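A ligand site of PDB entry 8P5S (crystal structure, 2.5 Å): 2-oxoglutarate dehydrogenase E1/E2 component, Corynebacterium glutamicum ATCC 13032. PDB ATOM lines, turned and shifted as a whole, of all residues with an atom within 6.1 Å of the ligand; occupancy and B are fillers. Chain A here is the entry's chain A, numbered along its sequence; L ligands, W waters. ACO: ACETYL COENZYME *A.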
ATOM      1  N   LEU A 731      -7.817  -1.929   7.574  1.00  0.00           N
ATOM      2  CA  LEU A 731      -7.146  -0.725   8.039  1.00  0.00           C
ATOM      3  C   LEU A 731      -8.157   0.283   8.594  1.00  0.00           C
ATOM      4  O   LEU A 731      -9.255   0.407   8.057  1.00  0.00           O
ATOM      5  CB  LEU A 731      -6.335  -0.072   6.899  1.00  0.00           C
ATOM      6  CG  LEU A 731      -5.314  -0.948   6.196  1.00  0.00           C
ATOM      7  CD1 LEU A 731      -4.550  -0.152   5.163  1.00  0.00           C
ATOM      8  CD2 LEU A 731      -4.336  -1.578   7.193  1.00  0.00           C
ATOM      9  N   PRO A 732      -7.805   0.996   9.673  1.00  0.00           N
ATOM     10  CA  PRO A 732      -8.747   1.989  10.223  1.00  0.00           C
ATOM     11  C   PRO A 732      -8.750   3.296   9.408  1.00  0.00           C
ATOM     12  O   PRO A 732      -8.235   4.320   9.864  1.00  0.00           O
ATOM     13  CB  PRO A 732      -8.224   2.215  11.636  1.00  0.00           C
ATOM     14  CG  PRO A 732      -6.750   1.970  11.539  1.00  0.00           C
ATOM     15  CD  PRO A 732      -6.559   0.936  10.453  1.00  0.00           C
ATOM     16  N   HIS A 733      -9.325   3.267   8.203  1.00  0.00           N
ATOM     17  CA  HIS A 733      -9.412   4.427   7.340  1.00  0.00           C
ATOM     18  C   HIS A 733     -10.361   5.454   7.939  1.00  0.00           C
ATOM     19  O   HIS A 733     -11.462   5.100   8.381  1.00  0.00           O
ATOM     20  CB  HIS A 733      -9.901   4.019   5.934  1.00  0.00           C
ATOM     21  CG  HIS A 733      -8.916   3.188   5.162  1.00  0.00           C
ATOM     22  ND1 HIS A 733      -7.739   3.722   4.671  1.00  0.00           N
ATOM     23  CD2 HIS A 733      -8.993   1.882   4.801  1.00  0.00           C
ATOM     24  CE1 HIS A 733      -7.128   2.737   4.048  1.00  0.00           C
ATOM     25  NE2 HIS A 733      -7.839   1.601   4.096  1.00  0.00           N
ATOM     26  N   GLY A 734      -9.930   6.703   7.989  1.00  0.00           N
ATOM     27  CA  GLY A 734     -10.734   7.787   8.529  1.00  0.00           C
ATOM     28  C   GLY A 734     -10.830   7.811  10.051  1.00  0.00           C
ATOM     29  O   GLY A 734     -11.743   8.451  10.597  1.00  0.00           O
ATOM     30  N   LEU A 735      -9.909   7.134  10.751  1.00  0.00           N
ATOM     31  CA  LEU A 735      -9.918   7.129  12.220  1.00  0.00           C
ATOM     32  C   LEU A 735      -9.097   8.309  12.733  1.00  0.00           C
ATOM     33  O   LEU A 735      -7.952   8.481  12.319  1.00  0.00           O
ATOM     34  CB  LEU A 735      -9.377   5.792  12.775  1.00  0.00           C
ATOM     35  CG  LEU A 735      -9.428   5.641  14.307  1.00  0.00           C
ATOM     36  CD1 LEU A 735     -10.866   5.674  14.815  1.00  0.00           C
ATOM     37  CD2 LEU A 735      -8.763   4.357  14.770  1.00  0.00           C
ATOM     38  N   THR A 939       2.893  -4.644  11.840  1.00  0.00           N
ATOM     39  CA  THR A 939       3.283  -3.259  11.577  1.00  0.00           C
ATOM     40  C   THR A 939       4.636  -3.001  12.218  1.00  0.00           C
ATOM     41  O   THR A 939       4.802  -3.288  13.399  1.00  0.00           O
ATOM     42  CB  THR A 939       2.239  -2.281  12.106  1.00  0.00           C
ATOM     43  OG1 THR A 939       0.962  -2.591  11.565  1.00  0.00           O
ATOM     44  CG2 THR A 939       2.573  -0.839  11.801  1.00  0.00           C
ATOM     45  N   ARG A 955      -3.397   4.533  17.188  1.00  0.00           N
ATOM     46  CA  ARG A 955      -4.047   3.982  16.009  1.00  0.00           C
ATOM     47  C   ARG A 955      -4.129   2.462  16.122  1.00  0.00           C
ATOM     48  O   ARG A 955      -5.166   1.885  15.829  1.00  0.00           O
ATOM     49  CB  ARG A 955      -3.310   4.384  14.731  1.00  0.00           C
ATOM     50  CG  ARG A 955      -4.040   3.963  13.476  1.00  0.00           C
ATOM     51  CD  ARG A 955      -3.259   4.295  12.223  1.00  0.00           C
ATOM     52  NE  ARG A 955      -2.056   3.476  12.111  1.00  0.00           N
ATOM     53  CZ  ARG A 955      -1.115   3.659  11.202  1.00  0.00           C
ATOM     54  NH1 ARG A 955      -1.218   4.630  10.298  1.00  0.00           N
ATOM     55  NH2 ARG A 955      -0.039   2.877  11.179  1.00  0.00           N
ATOM     56  N   SER A 959      -7.934   0.570  16.610  1.00  0.00           N
ATOM     57  CA  SER A 959      -8.330  -0.042  15.345  1.00  0.00           C
ATOM     58  C   SER A 959      -8.794  -1.472  15.553  1.00  0.00           C
ATOM     59  O   SER A 959      -8.594  -2.044  16.629  1.00  0.00           O
ATOM     60  CB  SER A 959      -7.152  -0.030  14.377  1.00  0.00           C
ATOM     61  OG  SER A 959      -6.119  -0.888  14.846  1.00  0.00           O
ATOM     62  N   LEU A 961      -7.456  -3.767  13.517  1.00  0.00           N
ATOM     63  CA  LEU A 961      -6.391  -4.505  12.866  1.00  0.00           C
ATOM     64  C   LEU A 961      -5.656  -5.272  13.948  1.00  0.00           C
ATOM     65  O   LEU A 961      -4.753  -4.759  14.602  1.00  0.00           O
ATOM     66  CB  LEU A 961      -5.452  -3.562  12.080  1.00  0.00           C
ATOM     67  CG  LEU A 961      -4.396  -4.262  11.227  1.00  0.00           C
ATOM     68  CD1 LEU A 961      -5.030  -5.209  10.209  1.00  0.00           C
ATOM     69  CD2 LEU A 961      -3.533  -3.273  10.525  1.00  0.00           C
ATOM     70  N   LYS A 991      -4.111  12.432  12.552  1.00  0.00           N
ATOM     71  CA  LYS A 991      -3.691  11.064  12.278  1.00  0.00           C
ATOM     72  C   LYS A 991      -2.171  10.858  12.451  1.00  0.00           C
ATOM     73  O   LYS A 991      -1.444  11.803  12.746  1.00  0.00           O
ATOM     74  CB  LYS A 991      -4.097  10.684  10.842  1.00  0.00           C
ATOM     75  CG  LYS A 991      -5.564  10.929  10.523  1.00  0.00           C
ATOM     76  CD  LYS A 991      -5.953  10.402   9.165  1.00  0.00           C
ATOM     77  CE  LYS A 991      -7.407  10.678   8.872  1.00  0.00           C
ATOM     78  NZ  LYS A 991      -8.287  10.150   9.945  1.00  0.00           N
ATOM     79  N   PHE A 992      -1.711   9.598  12.293  1.00  0.00           N
ATOM     80  CA  PHE A 992      -0.300   9.193  12.296  1.00  0.00           C
ATOM     81  C   PHE A 992       0.253   9.454  10.905  1.00  0.00           C
ATOM     82  O   PHE A 992      -0.428   9.222   9.902  1.00  0.00           O
ATOM     83  CB  PHE A 992      -0.146   7.708  12.696  1.00  0.00           C
ATOM     84  CG  PHE A 992       1.135   7.018  12.260  1.00  0.00           C
ATOM     85  CD1 PHE A 992       2.283   7.100  13.013  1.00  0.00           C
ATOM     86  CD2 PHE A 992       1.170   6.264  11.098  1.00  0.00           C
ATOM     87  CE1 PHE A 992       3.450   6.471  12.611  1.00  0.00           C
ATOM     88  CE2 PHE A 992       2.336   5.634  10.696  1.00  0.00           C
ATOM     89  CZ  PHE A 992       3.466   5.732  11.467  1.00  0.00           C
ATOM     90  N   GLN A 993       1.496   9.905  10.851  1.00  0.00           N
ATOM     91  CA  GLN A 993       2.142  10.180   9.580  1.00  0.00           C
ATOM     92  C   GLN A 993       3.086   9.065   9.227  1.00  0.00           C
ATOM     93  O   GLN A 993       3.934   8.703  10.023  1.00  0.00           O
ATOM     94  CB  GLN A 993       2.882  11.521   9.658  1.00  0.00           C
ATOM     95  CG  GLN A 993       1.953  12.704   9.812  1.00  0.00           C
ATOM     96  CD  GLN A 993       2.694  13.896  10.339  1.00  0.00           C
ATOM     97  OE1 GLN A 993       3.373  14.611   9.597  1.00  0.00           O
ATOM     98  NE2 GLN A 993       2.584  14.122  11.634  1.00  0.00           N
ATOM     99  N   SER A 994       2.936   8.500   8.024  1.00  0.00           N
ATOM    100  CA  SER A 994       3.803   7.448   7.521  1.00  0.00           C
ATOM    101  C   SER A 994       5.116   8.043   7.062  1.00  0.00           C
ATOM    102  O   SER A 994       6.172   7.471   7.287  1.00  0.00           O
ATOM    103  CB  SER A 994       3.127   6.711   6.367  1.00  0.00           C
ATOM    104  OG  SER A 994       2.269   5.695   6.837  1.00  0.00           O
ATOM    105  N   VAL A 995       5.040   9.186   6.357  1.00  0.00           N
ATOM    106  CA  VAL A 995       6.222   9.887   5.909  1.00  0.00           C
ATOM    107  C   VAL A 995       6.101  11.339   6.351  1.00  0.00           C
ATOM    108  O   VAL A 995       5.018  11.927   6.319  1.00  0.00           O
ATOM    109  CB  VAL A 995       6.509   9.767   4.393  1.00  0.00           C
ATOM    110  CG1 VAL A 995       6.428   8.309   3.930  1.00  0.00           C
ATOM    111  CG2 VAL A 995       5.595  10.645   3.564  1.00  0.00           C
ATOM    112  N   MET A1040       6.954   4.643   9.087  1.00  0.00           N
ATOM    113  CA  MET A1040       6.443   3.280   9.037  1.00  0.00           C
ATOM    114  C   MET A1040       7.239   2.496   8.006  1.00  0.00           C
ATOM    115  O   MET A1040       7.276   2.905   6.853  1.00  0.00           O
ATOM    116  CB  MET A1040       4.933   3.258   8.685  1.00  0.00           C
ATOM    117  CG  MET A1040       4.330   1.863   8.772  1.00  0.00           C
ATOM    118  SD  MET A1040       2.835   1.626   7.774  1.00  0.00           S
ATOM    119  CE  MET A1040       1.794   2.737   8.495  1.00  0.00           C
ATOM    120  N   HIS A1042       7.071  -1.222   7.565  1.00  0.00           N
ATOM    121  CA  HIS A1042       6.206  -2.221   6.978  1.00  0.00           C
ATOM    122  C   HIS A1042       4.798  -2.081   7.535  1.00  0.00           C
ATOM    123  O   HIS A1042       4.638  -2.069   8.754  1.00  0.00           O
ATOM    124  CB  HIS A1042       6.715  -3.654   7.192  1.00  0.00           C
ATOM    125  CG  HIS A1042       5.868  -4.673   6.498  1.00  0.00           C
ATOM    126  ND1 HIS A1042       4.823  -5.311   7.144  1.00  0.00           N
ATOM    127  CD2 HIS A1042       5.883  -5.057   5.206  1.00  0.00           C
ATOM    128  CE1 HIS A1042       4.266  -6.093   6.236  1.00  0.00           C
ATOM    129  NE2 HIS A1042       4.868  -5.973   5.047  1.00  0.00           N
ATOM    130  N   PRO A1043       3.761  -2.033   6.690  1.00  0.00           N
ATOM    131  CA  PRO A1043       3.837  -2.053   5.213  1.00  0.00           C
ATOM    132  C   PRO A1043       4.504  -0.799   4.647  1.00  0.00           C
ATOM    133  O   PRO A1043       4.609   0.220   5.318  1.00  0.00           O
ATOM    134  CB  PRO A1043       2.375  -2.204   4.771  1.00  0.00           C
ATOM    135  CG  PRO A1043       1.534  -1.828   5.957  1.00  0.00           C
ATOM    136  CD  PRO A1043       2.377  -1.947   7.191  1.00  0.00           C
ATOM    137  N   ILE A1044       5.045  -0.921   3.423  1.00  0.00           N
ATOM    138  CA  ILE A1044       5.729   0.189   2.782  1.00  0.00           C
ATOM    139  C   ILE A1044       4.702   1.223   2.361  1.00  0.00           C
ATOM    140  O   ILE A1044       3.816   0.928   1.586  1.00  0.00           O
ATOM    141  CB  ILE A1044       6.584  -0.257   1.576  1.00  0.00           C
ATOM    142  CG1 ILE A1044       7.687  -1.221   1.998  1.00  0.00           C
ATOM    143  CG2 ILE A1044       7.175   0.948   0.843  1.00  0.00           C
ATOM    144  CD1 ILE A1044       8.373  -1.874   0.847  1.00  0.00           C
ATOM    145  N   PRO A1045       4.823   2.451   2.885  1.00  0.00           N
ATOM    146  CA  PRO A1045       3.888   3.499   2.462  1.00  0.00           C
ATOM    147  C   PRO A1045       4.381   4.101   1.157  1.00  0.00           C
ATOM    148  O   PRO A1045       4.841   5.232   1.122  1.00  0.00           O
ATOM    149  CB  PRO A1045       3.965   4.499   3.618  1.00  0.00           C
ATOM    150  CG  PRO A1045       5.373   4.374   4.121  1.00  0.00           C
ATOM    151  CD  PRO A1045       5.840   2.969   3.820  1.00  0.00           C
ATOM    152  N   PHE A1046       4.274   3.331   0.060  1.00  0.00           N
ATOM    153  CA  PHE A1046       4.748   3.709  -1.258  1.00  0.00           C
ATOM    154  C   PHE A1046       3.940   4.865  -1.870  1.00  0.00           C
ATOM    155  O   PHE A1046       4.501   5.612  -2.657  1.00  0.00           O
ATOM    156  CB  PHE A1046       4.765   2.498  -2.210  1.00  0.00           C
ATOM    157  CG  PHE A1046       3.407   1.928  -2.552  1.00  0.00           C
ATOM    158  CD1 PHE A1046       2.748   1.082  -1.671  1.00  0.00           C
ATOM    159  CD2 PHE A1046       2.792   2.240  -3.748  1.00  0.00           C
ATOM    160  CE1 PHE A1046       1.497   0.576  -1.981  1.00  0.00           C
ATOM    161  CE2 PHE A1046       1.540   1.726  -4.062  1.00  0.00           C
ATOM    162  CZ  PHE A1046       0.902   0.891  -3.186  1.00  0.00           C
ATOM    163  N   ASN A1047       2.663   5.031  -1.494  1.00  0.00           N
ATOM    164  CA  ASN A1047       1.851   6.124  -2.015  1.00  0.00           C
ATOM    165  C   ASN A1047       2.283   7.453  -1.413  1.00  0.00           C
ATOM    166  O   ASN A1047       2.365   8.456  -2.132  1.00  0.00           O
ATOM    167  CB  ASN A1047       0.376   5.881  -1.742  1.00  0.00           C
ATOM    168  CG  ASN A1047      -0.157   4.677  -2.477  1.00  0.00           C
ATOM    169  OD1 ASN A1047      -0.131   4.630  -3.715  1.00  0.00           O
ATOM    170  ND2 ASN A1047      -0.629   3.678  -1.735  1.00  0.00           N
ATOM    171  N   ARG A1048       2.607   7.472  -0.110  1.00  0.00           N
ATOM    172  CA  ARG A1048       3.050   8.691   0.563  1.00  0.00           C
ATOM    173  C   ARG A1048       4.484   9.049   0.165  1.00  0.00           C
ATOM    174  O   ARG A1048       4.798  10.240   0.076  1.00  0.00           O
ATOM    175  CB  ARG A1048       2.903   8.579   2.077  1.00  0.00           C
ATOM    176  CG  ARG A1048       1.456   8.405   2.557  1.00  0.00           C
ATOM    177  CD  ARG A1048       0.519   9.554   2.180  1.00  0.00           C
ATOM    178  NE  ARG A1048       0.093   9.523   0.781  1.00  0.00           N
ATOM    179  CZ  ARG A1048      -0.944   8.836   0.318  1.00  0.00           C
ATOM    180  NH1 ARG A1048      -1.694   8.107   1.151  1.00  0.00           N
ATOM    181  NH2 ARG A1048      -1.255   8.852  -0.968  1.00  0.00           N
ATOM    182  N   ILE A1049       5.348   8.051  -0.093  1.00  0.00           N
ATOM    183  CA  ILE A1049       6.710   8.292  -0.557  1.00  0.00           C
ATOM    184  C   ILE A1049       6.654   8.820  -2.000  1.00  0.00           C
ATOM    185  O   ILE A1049       7.422   9.718  -2.361  1.00  0.00           O
ATOM    186  CB  ILE A1049       7.584   7.025  -0.443  1.00  0.00           C
ATOM    187  CG1 ILE A1049       7.827   6.671   1.018  1.00  0.00           C
ATOM    188  CG2 ILE A1049       8.908   7.187  -1.163  1.00  0.00           C
ATOM    189  CD1 ILE A1049       8.349   5.277   1.218  1.00  0.00           C
HETATM  190  N1A ACO L   1      -1.932   0.113  10.511  1.00  0.00           N
HETATM  191  C2A ACO L   1      -3.065   0.821  10.465  1.00  0.00           C
HETATM  192  N3A ACO L   1      -3.479   1.688   9.537  1.00  0.00           N
HETATM  193  C4A ACO L   1      -2.585   1.791   8.547  1.00  0.00           C
HETATM  194  C5A ACO L   1      -1.380   1.121   8.447  1.00  0.00           C
HETATM  195  C6A ACO L   1      -1.047   0.230   9.493  1.00  0.00           C
HETATM  196  N6A ACO L   1       0.052  -0.521   9.518  1.00  0.00           N
HETATM  197  N7A ACO L   1      -0.706   1.474   7.289  1.00  0.00           N
HETATM  198  C8A ACO L   1      -1.508   2.344   6.723  1.00  0.00           C
HETATM  199  N9A ACO L   1      -2.666   2.585   7.421  1.00  0.00           N
HETATM  200  C1B ACO L   1      -3.745   3.477   7.033  1.00  0.00           C
HETATM  201  C2B ACO L   1      -3.575   4.923   7.526  1.00  0.00           C
HETATM  202  O2B ACO L   1      -4.180   5.107   8.797  1.00  0.00           O
HETATM  203  C3B ACO L   1      -4.350   5.685   6.440  1.00  0.00           C
HETATM  204  O3B ACO L   1      -5.761   5.828   6.725  1.00  0.00           O
HETATM  205  P3B ACO L   1      -6.636   7.019   6.049  1.00  0.00           P
HETATM  206  O7A ACO L   1      -7.497   6.351   4.997  1.00  0.00           O
HETATM  207  O8A ACO L   1      -7.460   7.593   7.183  1.00  0.00           O
HETATM  208  O9A ACO L   1      -5.661   8.015   5.453  1.00  0.00           O
HETATM  209  C4B ACO L   1      -4.111   4.869   5.180  1.00  0.00           C
HETATM  210  O4B ACO L   1      -3.783   3.527   5.617  1.00  0.00           O
HETATM  211  C5B ACO L   1      -3.062   5.368   4.208  1.00  0.00           C
HETATM  212  O5B ACO L   1      -1.717   5.093   4.642  1.00  0.00           O
HETATM  213  P1A ACO L   1      -0.555   6.131   4.257  1.00  0.00           P
HETATM  214  O1A ACO L   1       0.221   6.399   5.478  1.00  0.00           O
HETATM  215  O2A ACO L   1      -1.163   7.283   3.540  1.00  0.00           O
HETATM  216  O3A ACO L   1       0.368   5.310   3.235  1.00  0.00           O
HETATM  217  P2A ACO L   1       0.237   4.516   1.853  1.00  0.00           P
HETATM  218  O4A ACO L   1      -1.081   4.769   1.245  1.00  0.00           O
HETATM  219  O5A ACO L   1       1.446   4.760   1.023  1.00  0.00           O
HETATM  220  O6A ACO L   1       0.212   3.028   2.443  1.00  0.00           O
HETATM  221  CBP ACO L   1      -0.030   0.639   2.049  1.00  0.00           C
HETATM  222  CCP ACO L   1       0.800   1.895   1.785  1.00  0.00           C
HETATM  223  CDP ACO L   1       0.813  -0.597   1.738  1.00  0.00           C
HETATM  224  CEP ACO L   1      -0.461   0.617   3.519  1.00  0.00           C
HETATM  225  CAP ACO L   1      -1.291   0.659   1.141  1.00  0.00           C
HETATM  226  O   HOH W   1      -0.138   5.512   7.821  1.00  0.00           O
HETATM  227  O   HOH W   2      -1.914  -0.310  13.481  1.00  0.00           O
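An oxygen (O4A) of the ligand sits at hydrogen-bond distance from the side-chain amide nitrogen (ND2) of Asn 1047 (3.2 Å).
O7A of the ligand is in hydrogen-bond range of ND1 of His 733 (2.7 Å).
The guanidinium group (NH1) of Arg 1048 lies within salt-bridge range of an oxygen (O2A) of the ligand (2.6 Å).
The side-chain hydroxyl (OG) of Ser 994 sits at hydrogen-bond distance from an oxygen (O1A) of the ligand (2.6 Å).
The backbone NH (N) of Gly 734 is in hydrogen-bond range of an oxygen (O8A) of the ligand (2.7 Å).
NZ of Lys 991 is in salt-bridge range of O8A of the ligand (3.9 Å).
The side-chain hydroxyl (OG1) of Thr 939 lies within hydrogen-bond range of a nitrogen (N6A) of the ligand (3.1 Å).
The backbone NH (N) of Asn 1047 lies within hydrogen-bond range of an oxygen (O5A) of the ligand (2.8 Å).
N of Phe 1046 is in hydrogen-bond range of O5A of the ligand (3.3 Å).
NH1 of Arg 955 is in hydrogen-bond range of O2B of the ligand, at 3.4 Å.
An oxygen (O5A) of the ligand sits at hydrogen-bond distance from the backbone NH (N) of Arg 1048 (3.2 Å).
Water W1 lies within hydrogen-bond range of O1A of the ligand, OG of Ser 994 and NH1 of Arg 955.
NZ of Lys 991 is in hydrogen-bond range of O of Leu 735 (2.9 Å).
The backbone carbonyl oxygen (O) of Ser 994 is in hydrogen-bond range of the backbone NH (N) of Met 1040 (3.4 Å).
The backbone carbonyl oxygen (O) of Arg 955 is in hydrogen-bond range of the side-chain hydroxyl (OG) of Ser 959, at 3.1 Å.
N of Leu 961 sits close to OG of Ser 959, 3.4 Å away.
N7A of the ligand sits close to SD of Met 1040.
O5A of the ligand sits close to O of Pro 1045.
Merely in contact with the ligand: Ile 1044, Pro 732, Pro 1043, Leu 961 and Leu 731.
Hydrophobic or aromatic side chains that line the ligand: Leu 731, Pro 732, His 733, Leu 961, Met 1040, Pro 1043, Pro 1045 and Phe 1046.
Of the 23 residues printed, 16 come within 4 Å of the ligand.
The nearest printed residue that does not touch the ligand is Leu 735 (4.4 Å).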
